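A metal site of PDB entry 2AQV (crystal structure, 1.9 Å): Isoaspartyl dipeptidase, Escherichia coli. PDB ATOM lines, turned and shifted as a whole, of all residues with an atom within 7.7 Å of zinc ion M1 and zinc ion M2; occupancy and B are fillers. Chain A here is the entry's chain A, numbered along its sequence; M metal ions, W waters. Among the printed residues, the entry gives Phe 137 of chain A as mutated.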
ATOM      1  N   HIS A  68     -19.317 -34.246  20.862  1.00  0.00           N
ATOM      2  CA  HIS A  68     -20.529 -33.590  21.280  1.00  0.00           C
ATOM      3  C   HIS A  68     -21.118 -34.240  22.523  1.00  0.00           C
ATOM      4  O   HIS A  68     -22.053 -35.041  22.444  1.00  0.00           O
ATOM      5  CB  HIS A  68     -21.556 -33.649  20.116  1.00  0.00           C
ATOM      6  CG  HIS A  68     -22.715 -32.729  20.353  1.00  0.00           C
ATOM      7  ND1 HIS A  68     -22.948 -31.693  19.492  1.00  0.00           N
ATOM      8  CD2 HIS A  68     -23.658 -32.676  21.354  1.00  0.00           C
ATOM      9  CE1 HIS A  68     -24.006 -31.030  19.931  1.00  0.00           C
ATOM     10  NE2 HIS A  68     -24.444 -31.601  21.048  1.00  0.00           N
ATOM     11  N   VAL A  69     -20.558 -33.891  23.678  1.00  0.00           N
ATOM     12  CA  VAL A  69     -20.988 -34.437  24.974  1.00  0.00           C
ATOM     13  C   VAL A  69     -21.244 -33.328  25.977  1.00  0.00           C
ATOM     14  O   VAL A  69     -20.425 -32.397  26.134  1.00  0.00           O
ATOM     15  CB  VAL A  69     -19.875 -35.279  25.641  1.00  0.00           C
ATOM     16  CG1 VAL A  69     -20.454 -35.992  26.875  1.00  0.00           C
ATOM     17  CG2 VAL A  69     -19.389 -36.363  24.680  1.00  0.00           C
ATOM     18  N   HIS A  70     -22.349 -33.468  26.686  1.00  0.00           N
ATOM     19  CA  HIS A  70     -22.722 -32.551  27.748  1.00  0.00           C
ATOM     20  C   HIS A  70     -22.121 -33.031  29.061  1.00  0.00           C
ATOM     21  O   HIS A  70     -22.818 -33.540  29.963  1.00  0.00           O
ATOM     22  CB  HIS A  70     -24.238 -32.488  27.877  1.00  0.00           C
ATOM     23  CG  HIS A  70     -24.746 -31.889  26.610  1.00  0.00           C
ATOM     24  ND1 HIS A  70     -24.941 -30.515  26.471  1.00  0.00           N
ATOM     25  CD2 HIS A  70     -25.055 -32.510  25.433  1.00  0.00           C
ATOM     26  CE1 HIS A  70     -25.337 -30.319  25.222  1.00  0.00           C
ATOM     27  NE2 HIS A  70     -25.443 -31.498  24.606  1.00  0.00           N
ATOM     28  N   LEU A 103     -19.621 -29.442  25.746  1.00  0.00           N
ATOM     29  CA  LEU A 103     -20.262 -28.209  25.308  1.00  0.00           C
ATOM     30  C   LEU A 103     -21.539 -28.053  26.122  1.00  0.00           C
ATOM     31  O   LEU A 103     -21.949 -28.966  26.837  1.00  0.00           O
ATOM     32  CB  LEU A 103     -20.672 -28.172  23.798  1.00  0.00           C
ATOM     33  CG  LEU A 103     -21.062 -29.538  23.202  1.00  0.00           C
ATOM     34  CD1 LEU A 103     -22.341 -30.048  23.815  1.00  0.00           C
ATOM     35  CD2 LEU A 103     -21.281 -29.386  21.719  1.00  0.00           C
ATOM     36  N   LEU A 104     -22.140 -26.877  25.978  1.00  0.00           N
ATOM     37  CA  LEU A 104     -23.408 -26.526  26.659  1.00  0.00           C
ATOM     38  C   LEU A 104     -24.474 -26.467  25.575  1.00  0.00           C
ATOM     39  O   LEU A 104     -24.150 -26.446  24.368  1.00  0.00           O
ATOM     40  CB  LEU A 104     -23.339 -25.194  27.437  1.00  0.00           C
ATOM     41  CG  LEU A 104     -22.184 -25.070  28.432  1.00  0.00           C
ATOM     42  CD1 LEU A 104     -22.204 -23.664  29.022  1.00  0.00           C
ATOM     43  CD2 LEU A 104     -22.348 -26.138  29.529  1.00  0.00           C
ATOM     44  N   GLY A 105     -25.721 -26.490  26.047  1.00  0.00           N
ATOM     45  CA  GLY A 105     -26.905 -26.472  25.190  1.00  0.00           C
ATOM     46  C   GLY A 105     -27.809 -25.280  25.466  1.00  0.00           C
ATOM     47  O   GLY A 105     -27.413 -24.109  25.547  1.00  0.00           O
ATOM     48  N   THR A 106     -29.082 -25.626  25.558  1.00  0.00           N
ATOM     49  CA  THR A 106     -30.165 -24.689  25.816  1.00  0.00           C
ATOM     50  C   THR A 106     -29.895 -23.782  27.024  1.00  0.00           C
ATOM     51  O   THR A 106     -29.926 -22.571  26.919  1.00  0.00           O
ATOM     52  CB  THR A 106     -31.526 -25.390  25.993  1.00  0.00           C
ATOM     53  OG1 THR A 106     -31.794 -26.155  24.846  1.00  0.00           O
ATOM     54  CG2 THR A 106     -32.622 -24.330  26.069  1.00  0.00           C
ATOM     55  N   PHE A 137     -26.306 -22.399  23.441  1.00  0.00           N
ATOM     56  CA  PHE A 137     -27.290 -21.994  22.428  1.00  0.00           C
ATOM     57  C   PHE A 137     -27.312 -20.475  22.189  1.00  0.00           C
ATOM     58  O   PHE A 137     -27.466 -20.022  21.062  1.00  0.00           O
ATOM     59  CB  PHE A 137     -28.723 -22.454  22.708  1.00  0.00           C
ATOM     60  CG  PHE A 137     -29.066 -23.902  22.329  1.00  0.00           C
ATOM     61  CD1 PHE A 137     -28.051 -24.852  22.199  1.00  0.00           C
ATOM     62  CD2 PHE A 137     -30.405 -24.304  22.127  1.00  0.00           C
ATOM     63  CE1 PHE A 137     -28.322 -26.180  21.875  1.00  0.00           C
ATOM     64  CE2 PHE A 137     -30.700 -25.625  21.792  1.00  0.00           C
ATOM     65  CZ  PHE A 137     -29.657 -26.551  21.669  1.00  0.00           C
ATOM     66  N   KCX A 162     -19.844 -22.738  20.468  1.00  0.00           N
ATOM     67  CA  KCX A 162     -21.082 -23.362  20.116  1.00  0.00           C
ATOM     68  CB  KCX A 162     -21.410 -24.317  21.281  1.00  0.00           C
ATOM     69  CG  KCX A 162     -22.852 -24.846  21.344  1.00  0.00           C
ATOM     70  CD  KCX A 162     -22.996 -26.034  20.407  1.00  0.00           C
ATOM     71  CE  KCX A 162     -24.389 -26.609  20.345  1.00  0.00           C
ATOM     72  NZ  KCX A 162     -24.727 -27.118  21.674  1.00  0.00           N
ATOM     73  C   KCX A 162     -22.190 -22.299  19.990  1.00  0.00           C
ATOM     74  O   KCX A 162     -22.125 -21.216  20.601  1.00  0.00           O
ATOM     75  CX  KCX A 162     -25.447 -28.337  21.364  1.00  0.00           C
ATOM     76  OQ1 KCX A 162     -25.735 -28.662  20.233  1.00  0.00           O
ATOM     77  OQ2 KCX A 162     -25.788 -28.980  22.458  1.00  0.00           O
ATOM     78  N   CYS A 163     -23.232 -22.632  19.221  1.00  0.00           N
ATOM     79  CA  CYS A 163     -24.461 -21.817  19.030  1.00  0.00           C
ATOM     80  C   CYS A 163     -25.638 -22.692  18.527  1.00  0.00           C
ATOM     81  O   CYS A 163     -25.457 -23.852  18.214  1.00  0.00           O
ATOM     82  CB  CYS A 163     -24.314 -20.597  18.087  1.00  0.00           C
ATOM     83  SG  CYS A 163     -24.224 -21.077  16.356  1.00  0.00           S
ATOM     84  N   ALA A 164     -26.853 -22.100  18.441  1.00  0.00           N
ATOM     85  CA  ALA A 164     -27.987 -22.795  17.923  1.00  0.00           C
ATOM     86  C   ALA A 164     -28.666 -21.890  16.914  1.00  0.00           C
ATOM     87  O   ALA A 164     -28.757 -20.666  17.117  1.00  0.00           O
ATOM     88  CB  ALA A 164     -29.044 -23.157  18.993  1.00  0.00           C
ATOM     89  N   ASP A 167     -34.023 -23.247  15.297  1.00  0.00           N
ATOM     90  CA  ASP A 167     -34.559 -24.044  16.347  1.00  0.00           C
ATOM     91  C   ASP A 167     -35.357 -23.115  17.238  1.00  0.00           C
ATOM     92  O   ASP A 167     -34.993 -21.954  17.475  1.00  0.00           O
ATOM     93  CB  ASP A 167     -33.367 -24.633  17.151  1.00  0.00           C
ATOM     94  CG  ASP A 167     -33.783 -25.606  18.235  1.00  0.00           C
ATOM     95  OD1 ASP A 167     -34.359 -25.287  19.261  1.00  0.00           O
ATOM     96  OD2 ASP A 167     -33.477 -26.837  17.942  1.00  0.00           O
ATOM     97  N   ARG A 169     -35.489 -23.039  20.206  1.00  0.00           N
ATOM     98  CA  ARG A 169     -34.783 -22.718  21.445  1.00  0.00           C
ATOM     99  C   ARG A 169     -33.638 -21.736  21.176  1.00  0.00           C
ATOM    100  O   ARG A 169     -32.790 -21.503  22.049  1.00  0.00           O
ATOM    101  CB  ARG A 169     -34.226 -23.946  22.169  1.00  0.00           C
ATOM    102  CG  ARG A 169     -35.320 -24.760  22.824  1.00  0.00           C
ATOM    103  CD  ARG A 169     -34.927 -26.218  23.009  1.00  0.00           C
ATOM    104  NE  ARG A 169     -34.645 -26.852  21.737  1.00  0.00           N
ATOM    105  CZ  ARG A 169     -34.054 -28.019  21.546  1.00  0.00           C
ATOM    106  NH1 ARG A 169     -33.621 -28.784  22.557  1.00  0.00           N
ATOM    107  NH2 ARG A 169     -33.895 -28.426  20.291  1.00  0.00           N
ATOM    108  N   VAL A 199     -19.705 -24.499  15.844  1.00  0.00           N
ATOM    109  CA  VAL A 199     -20.589 -25.650  15.803  1.00  0.00           C
ATOM    110  C   VAL A 199     -22.037 -25.190  15.927  1.00  0.00           C
ATOM    111  O   VAL A 199     -22.413 -24.495  16.916  1.00  0.00           O
ATOM    112  CB  VAL A 199     -20.247 -26.673  16.912  1.00  0.00           C
ATOM    113  CG1 VAL A 199     -21.254 -27.838  16.912  1.00  0.00           C
ATOM    114  CG2 VAL A 199     -18.802 -27.188  16.827  1.00  0.00           C
ATOM    115  N   PHE A 200     -22.865 -25.577  14.942  1.00  0.00           N
ATOM    116  CA  PHE A 200     -24.237 -25.134  15.003  1.00  0.00           C
ATOM    117  C   PHE A 200     -25.216 -26.241  15.324  1.00  0.00           C
ATOM    118  O   PHE A 200     -25.393 -27.138  14.524  1.00  0.00           O
ATOM    119  CB  PHE A 200     -24.646 -24.615  13.605  1.00  0.00           C
ATOM    120  CG  PHE A 200     -23.790 -23.490  13.083  1.00  0.00           C
ATOM    121  CD1 PHE A 200     -22.558 -23.767  12.486  1.00  0.00           C
ATOM    122  CD2 PHE A 200     -24.236 -22.173  13.153  1.00  0.00           C
ATOM    123  CE1 PHE A 200     -21.753 -22.735  11.995  1.00  0.00           C
ATOM    124  CE2 PHE A 200     -23.451 -21.131  12.626  1.00  0.00           C
ATOM    125  CZ  PHE A 200     -22.204 -21.412  12.078  1.00  0.00           C
ATOM    126  N   HIS A 201     -25.891 -26.116  16.466  1.00  0.00           N
ATOM    127  CA  HIS A 201     -26.945 -27.056  16.823  1.00  0.00           C
ATOM    128  C   HIS A 201     -28.049 -26.752  15.827  1.00  0.00           C
ATOM    129  O   HIS A 201     -28.516 -25.608  15.772  1.00  0.00           O
ATOM    130  CB  HIS A 201     -27.544 -26.812  18.259  1.00  0.00           C
ATOM    131  CG  HIS A 201     -28.974 -27.267  18.406  1.00  0.00           C
ATOM    132  ND1 HIS A 201     -29.305 -28.428  19.082  1.00  0.00           N
ATOM    133  CD2 HIS A 201     -30.139 -26.742  17.968  1.00  0.00           C
ATOM    134  CE1 HIS A 201     -30.628 -28.586  19.088  1.00  0.00           C
ATOM    135  NE2 HIS A 201     -31.162 -27.592  18.411  1.00  0.00           N
ATOM    136  N   MET A 202     -28.486 -27.731  15.057  1.00  0.00           N
ATOM    137  CA  MET A 202     -29.575 -27.438  14.121  1.00  0.00           C
ATOM    138  C   MET A 202     -30.903 -27.912  14.708  1.00  0.00           C
ATOM    139  O   MET A 202     -30.977 -28.997  15.289  1.00  0.00           O
ATOM    140  CB  MET A 202     -29.393 -28.224  12.799  1.00  0.00           C
ATOM    141  CG  MET A 202     -28.140 -27.911  12.010  1.00  0.00           C
ATOM    142  SD  MET A 202     -27.847 -26.150  11.756  1.00  0.00           S
ATOM    143  CE  MET A 202     -29.310 -25.751  10.748  1.00  0.00           C
ATOM    144  N   GLY A 203     -31.971 -27.148  14.542  1.00  0.00           N
ATOM    145  CA  GLY A 203     -33.254 -27.594  15.019  1.00  0.00           C
ATOM    146  C   GLY A 203     -34.119 -27.932  13.794  1.00  0.00           C
ATOM    147  O   GLY A 203     -33.606 -28.143  12.696  1.00  0.00           O
ATOM    148  N   THR A 229     -24.489 -29.672  13.147  1.00  0.00           N
ATOM    149  CA  THR A 229     -24.679 -30.921  13.849  1.00  0.00           C
ATOM    150  C   THR A 229     -26.163 -31.316  13.926  1.00  0.00           C
ATOM    151  O   THR A 229     -26.990 -30.465  13.639  1.00  0.00           O
ATOM    152  CB  THR A 229     -23.888 -30.985  15.169  1.00  0.00           C
ATOM    153  OG1 THR A 229     -24.034 -32.299  15.631  1.00  0.00           O
ATOM    154  CG2 THR A 229     -24.462 -30.015  16.191  1.00  0.00           C
ATOM    155  N   HIS A 230     -26.497 -32.598  14.213  1.00  0.00           N
ATOM    156  CA  HIS A 230     -27.870 -33.119  14.256  1.00  0.00           C
ATOM    157  C   HIS A 230     -28.524 -33.057  12.857  1.00  0.00           C
ATOM    158  O   HIS A 230     -29.732 -32.904  12.749  1.00  0.00           O
ATOM    159  CB  HIS A 230     -28.816 -32.333  15.213  1.00  0.00           C
ATOM    160  CG  HIS A 230     -28.207 -31.972  16.521  1.00  0.00           C
ATOM    161  ND1 HIS A 230     -27.501 -32.919  17.273  1.00  0.00           N
ATOM    162  CD2 HIS A 230     -28.171 -30.796  17.177  1.00  0.00           C
ATOM    163  CE1 HIS A 230     -27.066 -32.319  18.367  1.00  0.00           C
ATOM    164  NE2 HIS A 230     -27.439 -31.054  18.325  1.00  0.00           N
ATOM    165  N   ARG A 233     -31.711 -35.123  11.733  1.00  0.00           N
ATOM    166  CA  ARG A 233     -32.966 -34.860  12.483  1.00  0.00           C
ATOM    167  C   ARG A 233     -34.232 -34.706  11.658  1.00  0.00           C
ATOM    168  O   ARG A 233     -35.350 -34.940  12.142  1.00  0.00           O
ATOM    169  CB  ARG A 233     -32.854 -33.738  13.494  1.00  0.00           C
ATOM    170  CG  ARG A 233     -32.579 -32.380  12.832  1.00  0.00           C
ATOM    171  CD  ARG A 233     -32.570 -31.218  13.828  1.00  0.00           C
ATOM    172  NE  ARG A 233     -33.595 -31.417  14.846  1.00  0.00           N
ATOM    173  CZ  ARG A 233     -33.431 -31.434  16.174  1.00  0.00           C
ATOM    174  NH1 ARG A 233     -32.254 -31.252  16.816  1.00  0.00           N
ATOM    175  NH2 ARG A 233     -34.509 -31.662  16.891  1.00  0.00           N
ATOM    176  N   THR A 254     -25.719 -37.234  14.353  1.00  0.00           N
ATOM    177  CA  THR A 254     -25.893 -37.569  15.748  1.00  0.00           C
ATOM    178  C   THR A 254     -26.367 -38.999  15.902  1.00  0.00           C
ATOM    179  O   THR A 254     -27.409 -39.362  15.343  1.00  0.00           O
ATOM    180  CB  THR A 254     -26.860 -36.586  16.454  1.00  0.00           C
ATOM    181  OG1 THR A 254     -26.421 -35.268  16.174  1.00  0.00           O
ATOM    182  CG2 THR A 254     -26.967 -36.814  17.972  1.00  0.00           C
ATOM    183  N   SER A 284     -22.253 -38.146  19.729  1.00  0.00           N
ATOM    184  CA  SER A 284     -23.346 -38.694  20.453  1.00  0.00           C
ATOM    185  C   SER A 284     -24.422 -37.772  20.982  1.00  0.00           C
ATOM    186  O   SER A 284     -25.586 -38.216  21.093  1.00  0.00           O
ATOM    187  CB  SER A 284     -22.858 -39.595  21.618  1.00  0.00           C
ATOM    188  OG  SER A 284     -22.241 -38.788  22.614  1.00  0.00           O
ATOM    189  N   ASP A 285     -24.042 -36.559  21.381  1.00  0.00           N
ATOM    190  CA  ASP A 285     -24.958 -35.678  22.086  1.00  0.00           C
ATOM    191  C   ASP A 285     -25.239 -36.333  23.462  1.00  0.00           C
ATOM    192  O   ASP A 285     -26.273 -36.126  24.114  1.00  0.00           O
ATOM    193  CB  ASP A 285     -26.276 -35.366  21.343  1.00  0.00           C
ATOM    194  CG  ASP A 285     -26.846 -34.055  21.869  1.00  0.00           C
ATOM    195  OD1 ASP A 285     -26.290 -33.412  22.712  1.00  0.00           O
ATOM    196  OD2 ASP A 285     -28.001 -33.683  21.389  1.00  0.00           O
ATOM    197  N   GLY A 286     -24.280 -37.175  23.900  1.00  0.00           N
ATOM    198  CA  GLY A 286     -24.389 -37.901  25.166  1.00  0.00           C
ATOM    199  C   GLY A 286     -24.598 -36.979  26.377  1.00  0.00           C
ATOM    200  O   GLY A 286     -24.008 -35.887  26.516  1.00  0.00           O
ATOM    201  N   ASN A 287     -25.454 -37.467  27.268  1.00  0.00           N
ATOM    202  CA  ASN A 287     -25.823 -36.764  28.493  1.00  0.00           C
ATOM    203  C   ASN A 287     -26.783 -35.589  28.314  1.00  0.00           C
ATOM    204  O   ASN A 287     -27.024 -34.831  29.251  1.00  0.00           O
ATOM    205  CB  ASN A 287     -24.662 -36.426  29.419  1.00  0.00           C
ATOM    206  CG  ASN A 287     -24.787 -37.182  30.717  1.00  0.00           C
ATOM    207  OD1 ASN A 287     -25.205 -38.348  30.733  1.00  0.00           O
ATOM    208  ND2 ASN A 287     -24.401 -36.470  31.777  1.00  0.00           N
ATOM    209  N   GLY A 288     -27.341 -35.449  27.096  1.00  0.00           N
ATOM    210  CA  GLY A 288     -28.290 -34.385  26.782  1.00  0.00           C
ATOM    211  C   GLY A 288     -29.740 -34.742  27.157  1.00  0.00           C
ATOM    212  O   GLY A 288     -30.001 -35.703  27.891  1.00  0.00           O
HETATM  213 ZN    ZN M   1     -26.095 -31.162  22.480  1.00  0.00          ZN
HETATM  214 ZN    ZN M   2     -27.775 -29.802  19.979  1.00  0.00          ZN
HETATM  215  O   HOH W   1     -28.656 -30.783  22.218  1.00  0.00           O
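A ring nitrogen (ND1) of His 230 sits at hydrogen-bond distance from the side-chain hydroxyl of Thr 254, at 2.8 Å. NZ of KCX 162 is in hydrogen-bond range of the backbone carbonyl oxygen (O) of Leu 104, at 2.8 Å. The backbone carbonyl oxygen of His 68 is in hydrogen-bond range of the backbone NH of Gly 286, 3.4 Å away. NE2 of His 201 lies within hydrogen-bond range of NH2 of Arg 169, at 3.4 Å. O of Cys 163 sits at hydrogen-bond distance from N of His 201 (2.9 Å). A ring nitrogen (NE2) of His 201 lies within hydrogen-bond range of the side-chain carboxylate (OD2) of Asp 167, at 2.5 Å. O of Leu 103 is in hydrogen-bond range of ND1 of His 70 (3.4 Å). N of His 70 is in hydrogen-bond range of O of Gly 286 (2.9 Å).
Four residues have an atom within 4 Å of zinc ion M1: His 68, His 70, KCX 162 and Asp 285.
Of the 27 residues printed, 4 come within 4 Å of zinc ion M2.
Zinc ion M1 is bound by OQ2 of KCX 162 (2.2 Å), NE2 of His 68 (2.2 Å), NE2 of His 70 (2.2 Å) and OD1 of Asp 285 (2.3 Å). Zinc ion M1 has four donor atoms within binding distance. Slightly farther from zinc ion M1 lies water W1 (2.6 Å).
Zinc ion M2 is bound by NE2 of His 230, at 2.1 Å. A ring nitrogen (ND1) of His 201 binds zinc ion M2 (2.2 Å). Zinc ion M2 is bound by OQ1 of KCX 162, 2.4 Å away. Water W1 is bound to zinc ion M2 (2.6 Å). Zinc ion M2 has four donor atoms within binding distance.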
